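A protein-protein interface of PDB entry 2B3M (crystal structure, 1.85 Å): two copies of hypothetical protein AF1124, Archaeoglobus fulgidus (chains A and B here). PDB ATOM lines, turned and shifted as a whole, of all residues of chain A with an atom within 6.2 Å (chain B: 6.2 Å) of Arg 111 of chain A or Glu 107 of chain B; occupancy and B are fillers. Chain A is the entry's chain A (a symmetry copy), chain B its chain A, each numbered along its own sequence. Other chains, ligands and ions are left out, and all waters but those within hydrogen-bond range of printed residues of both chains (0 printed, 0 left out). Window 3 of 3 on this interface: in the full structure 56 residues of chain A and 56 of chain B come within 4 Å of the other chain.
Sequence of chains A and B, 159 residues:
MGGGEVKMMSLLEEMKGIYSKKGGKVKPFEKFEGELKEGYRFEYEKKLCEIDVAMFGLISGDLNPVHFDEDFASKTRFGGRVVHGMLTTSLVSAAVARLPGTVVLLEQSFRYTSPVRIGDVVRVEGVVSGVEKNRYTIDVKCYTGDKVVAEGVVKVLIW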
ATOM      1  N   SER A 109      12.535  13.792 -20.926  1.00  0.00           N
ATOM      2  CA  SER A 109      12.945  14.063 -22.310  1.00  0.00           C
ATOM      3  C   SER A 109      13.444  15.488 -22.323  1.00  0.00           C
ATOM      4  O   SER A 109      12.752  16.396 -21.865  1.00  0.00           O
ATOM      5  CB  SER A 109      11.759  13.908 -23.268  1.00  0.00           C
ATOM      6  OG  SER A 109      12.143  14.187 -24.614  1.00  0.00           O
ATOM      7  N   PHE A 110      14.681  15.676 -22.801  1.00  0.00           N
ATOM      8  CA  PHE A 110      15.279  17.005 -22.803  1.00  0.00           C
ATOM      9  C   PHE A 110      16.059  17.238 -24.056  1.00  0.00           C
ATOM     10  O   PHE A 110      16.633  16.300 -24.589  1.00  0.00           O
ATOM     11  CB  PHE A 110      16.241  17.190 -21.628  1.00  0.00           C
ATOM     12  CG  PHE A 110      15.507  17.439 -20.335  1.00  0.00           C
ATOM     13  CD1 PHE A 110      15.249  16.387 -19.489  1.00  0.00           C
ATOM     14  CD2 PHE A 110      14.972  18.704 -20.071  1.00  0.00           C
ATOM     15  CE1 PHE A 110      14.499  16.590 -18.306  1.00  0.00           C
ATOM     16  CE2 PHE A 110      14.231  18.937 -18.902  1.00  0.00           C
ATOM     17  CZ  PHE A 110      13.993  17.844 -18.026  1.00  0.00           C
ATOM     18  N   ARG A 111      16.061  18.496 -24.501  1.00  0.00           N
ATOM     19  CA  ARG A 111      16.935  18.943 -25.597  1.00  0.00           C
ATOM     20  C   ARG A 111      17.837  19.988 -24.986  1.00  0.00           C
ATOM     21  O   ARG A 111      17.369  20.863 -24.210  1.00  0.00           O
ATOM     22  CB  ARG A 111      16.108  19.576 -26.739  1.00  0.00           C
ATOM     23  CG  ARG A 111      16.954  20.247 -27.852  1.00  0.00           C
ATOM     24  CD  ARG A 111      16.023  20.712 -29.003  1.00  0.00           C
ATOM     25  NE  ARG A 111      16.536  21.949 -29.619  1.00  0.00           N
ATOM     26  CZ  ARG A 111      16.036  23.168 -29.387  1.00  0.00           C
ATOM     27  NH1 ARG A 111      14.992  23.320 -28.562  1.00  0.00           N
ATOM     28  NH2 ARG A 111      16.569  24.227 -29.984  1.00  0.00           N
ATOM     29  N   TYR A 112      19.134  19.874 -25.281  1.00  0.00           N
ATOM     30  CA  TYR A 112      20.134  20.771 -24.725  1.00  0.00           C
ATOM     31  C   TYR A 112      20.340  21.871 -25.751  1.00  0.00           C
ATOM     32  O   TYR A 112      20.633  21.572 -26.901  1.00  0.00           O
ATOM     33  CB  TYR A 112      21.433  20.005 -24.440  1.00  0.00           C
ATOM     34  CG  TYR A 112      21.155  18.963 -23.367  1.00  0.00           C
ATOM     35  CD1 TYR A 112      21.180  19.320 -22.012  1.00  0.00           C
ATOM     36  CD2 TYR A 112      20.814  17.674 -23.709  1.00  0.00           C
ATOM     37  CE1 TYR A 112      20.870  18.365 -21.004  1.00  0.00           C
ATOM     38  CE2 TYR A 112      20.488  16.716 -22.703  1.00  0.00           C
ATOM     39  CZ  TYR A 112      20.547  17.083 -21.372  1.00  0.00           C
ATOM     40  OH  TYR A 112      20.208  16.134 -20.400  1.00  0.00           O
ATOM     41  N   THR A 113      20.217  23.123 -25.311  1.00  0.00           N
ATOM     42  CA  THR A 113      20.081  24.264 -26.233  1.00  0.00           C
ATOM     43  C   THR A 113      21.306  25.181 -26.232  1.00  0.00           C
ATOM     44  O   THR A 113      21.593  25.848 -27.229  1.00  0.00           O
ATOM     45  CB  THR A 113      18.811  25.087 -25.888  1.00  0.00           C
ATOM     46  OG1 THR A 113      18.832  25.465 -24.511  1.00  0.00           O
ATOM     47  CG2 THR A 113      17.564  24.257 -26.119  1.00  0.00           C
ATOM     48  N   VAL A 149      19.094  26.649 -21.199  1.00  0.00           N
ATOM     49  CA  VAL A 149      20.177  25.698 -21.461  1.00  0.00           C
ATOM     50  C   VAL A 149      19.633  24.311 -21.731  1.00  0.00           C
ATOM     51  O   VAL A 149      20.300  23.489 -22.363  1.00  0.00           O
ATOM     52  CB  VAL A 149      21.284  25.689 -20.353  1.00  0.00           C
ATOM     53  CG1 VAL A 149      22.047  27.028 -20.339  1.00  0.00           C
ATOM     54  CG2 VAL A 149      20.673  25.308 -18.950  1.00  0.00           C
ATOM     55  N   ALA A 150      18.398  24.042 -21.271  1.00  0.00           N
ATOM     56  CA  ALA A 150      17.728  22.788 -21.595  1.00  0.00           C
ATOM     57  C   ALA A 150      16.217  22.955 -21.478  1.00  0.00           C
ATOM     58  O   ALA A 150      15.742  23.781 -20.689  1.00  0.00           O
ATOM     59  CB  ALA A 150      18.232  21.618 -20.723  1.00  0.00           C
ATOM     60  N   GLU A 151      15.472  22.226 -22.296  1.00  0.00           N
ATOM     61  CA  GLU A 151      14.012  22.268 -22.224  1.00  0.00           C
ATOM     62  C   GLU A 151      13.425  20.903 -22.493  1.00  0.00           C
ATOM     63  O   GLU A 151      13.968  20.126 -23.299  1.00  0.00           O
ATOM     64  CB  GLU A 151      13.396  23.336 -23.135  1.00  0.00           C
ATOM     65  CG  GLU A 151      13.745  23.254 -24.590  1.00  0.00           C
ATOM     66  CD  GLU A 151      13.456  24.578 -25.329  1.00  0.00           C
ATOM     67  OE1 GLU A 151      14.169  24.865 -26.307  1.00  0.00           O
ATOM     68  OE2 GLU A 151      12.538  25.340 -24.913  1.00  0.00           O
ATOM     69  N   GLY A 152      12.292  20.605 -21.857  1.00  0.00           N
ATOM     70  CA  GLY A 152      11.729  19.287 -22.041  1.00  0.00           C
ATOM     71  C   GLY A 152      10.549  19.047 -21.127  1.00  0.00           C
ATOM     72  O   GLY A 152       9.922  19.988 -20.651  1.00  0.00           O
ATOM     73  N   LEU B 105      26.248  15.704 -26.010  1.00  0.00           N
ATOM     74  CA  LEU B 105      24.841  15.309 -25.965  1.00  0.00           C
ATOM     75  C   LEU B 105      23.905  16.414 -26.457  1.00  0.00           C
ATOM     76  O   LEU B 105      23.985  17.554 -25.992  1.00  0.00           O
ATOM     77  CB  LEU B 105      24.470  14.894 -24.501  1.00  0.00           C
ATOM     78  CG  LEU B 105      23.082  14.312 -24.368  1.00  0.00           C
ATOM     79  CD1 LEU B 105      22.867  13.020 -25.191  1.00  0.00           C
ATOM     80  CD2 LEU B 105      22.797  14.023 -22.821  1.00  0.00           C
ATOM     81  N   LEU B 106      22.985  16.089 -27.380  1.00  0.00           N
ATOM     82  CA  LEU B 106      22.020  17.074 -27.863  1.00  0.00           C
ATOM     83  C   LEU B 106      20.587  16.861 -27.320  1.00  0.00           C
ATOM     84  O   LEU B 106      19.888  17.838 -27.066  1.00  0.00           O
ATOM     85  CB  LEU B 106      21.908  17.051 -29.393  1.00  0.00           C
ATOM     86  CG  LEU B 106      23.160  17.465 -30.189  1.00  0.00           C
ATOM     87  CD1 LEU B 106      22.799  17.441 -31.663  1.00  0.00           C
ATOM     88  CD2 LEU B 106      23.607  18.841 -29.771  1.00  0.00           C
ATOM     89  N   GLU B 107      20.186  15.601 -27.231  1.00  0.00           N
ATOM     90  CA  GLU B 107      18.820  15.213 -26.765  1.00  0.00           C
ATOM     91  C   GLU B 107      18.840  13.893 -26.065  1.00  0.00           C
ATOM     92  O   GLU B 107      19.631  13.005 -26.395  1.00  0.00           O
ATOM     93  CB  GLU B 107      17.833  15.117 -27.959  1.00  0.00           C
ATOM     94  CG  GLU B 107      17.843  16.351 -28.887  1.00  0.00           C
ATOM     95  CD  GLU B 107      16.841  16.308 -30.063  1.00  0.00           C
ATOM     96  OE1 GLU B 107      16.111  15.313 -30.204  1.00  0.00           O
ATOM     97  OE2 GLU B 107      16.801  17.288 -30.856  1.00  0.00           O
ATOM     98  N   GLN B 108      17.931  13.712 -25.078  1.00  0.00           N
ATOM     99  CA  GLN B 108      17.795  12.385 -24.489  1.00  0.00           C
ATOM    100  C   GLN B 108      16.338  12.232 -24.101  1.00  0.00           C
ATOM    101  O   GLN B 108      15.659  13.225 -23.787  1.00  0.00           O
ATOM    102  CB  GLN B 108      18.699  12.218 -23.255  1.00  0.00           C
ATOM    103  CG  GLN B 108      18.541  13.368 -22.268  1.00  0.00           C
ATOM    104  CD  GLN B 108      18.358  12.927 -20.865  1.00  0.00           C
ATOM    105  OE1 GLN B 108      18.195  11.714 -20.581  1.00  0.00           O
ATOM    106  NE2 GLN B 108      18.347  13.904 -19.943  1.00  0.00           N
ATOM    107  N   SER B 109      15.854  11.006 -24.176  1.00  0.00           N
ATOM    108  CA  SER B 109      14.461  10.738 -23.799  1.00  0.00           C
ATOM    109  C   SER B 109      14.432   9.311 -23.303  1.00  0.00           C
ATOM    110  O   SER B 109      14.904   8.404 -23.987  1.00  0.00           O
ATOM    111  CB  SER B 109      13.530  10.898 -25.006  1.00  0.00           C
ATOM    112  OG  SER B 109      12.175  10.621 -24.654  1.00  0.00           O
ATOM    113  N   VAL B 153      15.947   7.022 -26.405  1.00  0.00           N
ATOM    114  CA  VAL B 153      16.711   7.470 -27.586  1.00  0.00           C
ATOM    115  C   VAL B 153      17.573   8.650 -27.175  1.00  0.00           C
ATOM    116  O   VAL B 153      17.111   9.534 -26.405  1.00  0.00           O
ATOM    117  CB  VAL B 153      15.777   8.010 -28.680  1.00  0.00           C
ATOM    118  CG1 VAL B 153      16.593   8.383 -29.965  1.00  0.00           C
ATOM    119  CG2 VAL B 153      14.630   7.037 -28.991  1.00  0.00           C
ATOM    120  N   VAL B 154      18.797   8.720 -27.698  1.00  0.00           N
ATOM    121  CA  VAL B 154      19.573   9.929 -27.489  1.00  0.00           C
ATOM    122  C   VAL B 154      20.046  10.414 -28.863  1.00  0.00           C
ATOM    123  O   VAL B 154      20.098   9.616 -29.814  1.00  0.00           O
ATOM    124  CB  VAL B 154      20.792   9.730 -26.537  1.00  0.00           C
ATOM    125  CG1 VAL B 154      20.339   9.293 -25.116  1.00  0.00           C
ATOM    126  CG2 VAL B 154      21.815   8.721 -27.090  1.00  0.00           C
ATOM    127  N   LYS B 155      20.347  11.697 -28.932  1.00  0.00           N
ATOM    128  CA  LYS B 155      20.974  12.288 -30.139  1.00  0.00           C
ATOM    129  C   LYS B 155      22.253  12.949 -29.664  1.00  0.00           C
ATOM    130  O   LYS B 155      22.280  13.657 -28.636  1.00  0.00           O
ATOM    131  CB  LYS B 155      20.054  13.293 -30.819  1.00  0.00           C
ATOM    132  CG  LYS B 155      20.621  13.836 -32.206  1.00  0.00           C
ATOM    133  CD  LYS B 155      19.595  14.731 -32.938  1.00  0.00           C
ATOM    134  CE  LYS B 155      18.248  14.001 -33.116  1.00  0.00           C
ATOM    135  NZ  LYS B 155      17.404  14.752 -34.122  1.00  0.00           N
ATOM    136  N   VAL B 156      23.347  12.691 -30.387  1.00  0.00           N
ATOM    137  CA  VAL B 156      24.583  13.340 -30.037  1.00  0.00           C
ATOM    138  C   VAL B 156      25.174  14.009 -31.296  1.00  0.00           C
ATOM    139  O   VAL B 156      24.872  13.590 -32.410  1.00  0.00           O
ATOM    140  CB  VAL B 156      25.630  12.361 -29.455  1.00  0.00           C
ATOM    141  CG1 VAL B 156      25.162  11.729 -28.143  1.00  0.00           C
ATOM    142  CG2 VAL B 156      26.022  11.242 -30.470  1.00  0.00           C
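Hydrophobic or aromatic side chains of chain B that line the printed part of chain A: Leu 105.
Among the printed residues, 9 pairs touch across the chains.
The backbone NH (N) of Tyr 112 of chain A sits at hydrogen-bond distance from the backbone carbonyl oxygen (O) of Leu 106 of chain B (2.8 Å).
The backbone NH (N) of Phe 110 of chain A lies within hydrogen-bond range of the backbone carbonyl oxygen (O) of Gln 108 of chain B (2.8 Å).
The side-chain amide nitrogen (NE2) of Gln 108 of chain B is in hydrogen-bond range of the side-chain hydroxyl (OH) of Tyr 112 of chain A.
Among the printed residues, merely in contact across the chains: Ser 109 of chain A with Gln 108 of chain B (3.2 Å), Ser 109 of chain A with Ser 109 of chain B (3.6 Å), Phe 110 of chain A with Glu 107 of chain B (3.3 Å), Arg 111 of chain A with Leu 106 of chain B (3.5 Å), Arg 111 of chain A with Glu 107 of chain B (3.97 Å) and Tyr 112 of chain A with Leu 105 of chain B (3.5 Å).
N of Leu 106 of chain B lies within hydrogen-bond range of O of Lys 155 of chain B (2.8 Å).
The backbone NH of Lys 155 of chain B lies within hydrogen-bond range of the backbone carbonyl oxygen of Glu 107 of chain B (2.9 Å).
The backbone NH (N) of Ser 109 of chain B lies within hydrogen-bond range of the backbone carbonyl oxygen (O) of Val 153 of chain B (3.0 Å).
OE1 of Glu 151 of chain A is in salt-bridge range of NH1 of Arg 111 of chain A (2.9 Å).
Ser 109 of chain B touches its own counterpart, Ser 109 of chain A.
1 position is printed for both chains.
Arg 111 of chain A touches just these residues of chain B: Leu 106 (3.5 Å) and Glu 107 (3.97 Å).
Of chain A, only Phe 110 and Arg 111 come within 4 Å of Glu 107 of chain B.
Printed residues of chain A within 4 Å of Leu 105 of chain B: Tyr 112.
Printed residues of chain A within 4 Å of Leu 106 of chain B: Arg 111 (3.5 Å) and Tyr 112 (2.8 Å).
Printed residues of chain A within 4 Å of Gln 108 of chain B: Ser 109, Phe 110 and Tyr 112.
Lys 155 of chain B touches none of the printed residues of chain A.
Val 153 of chain B touches none of the printed residues of chain A.
The nearest residue of chain B that does not touch Arg 111 of chain A is Gln 108 of chain B (5.2 Å).
The nearest residue of chain A that does not touch Glu 107 of chain B is Tyr 112 of chain A (4.1 Å).
The nearest printed residue of chain A that does not touch Gln 108 of chain B is Arg 111 of chain A (5.2 Å).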
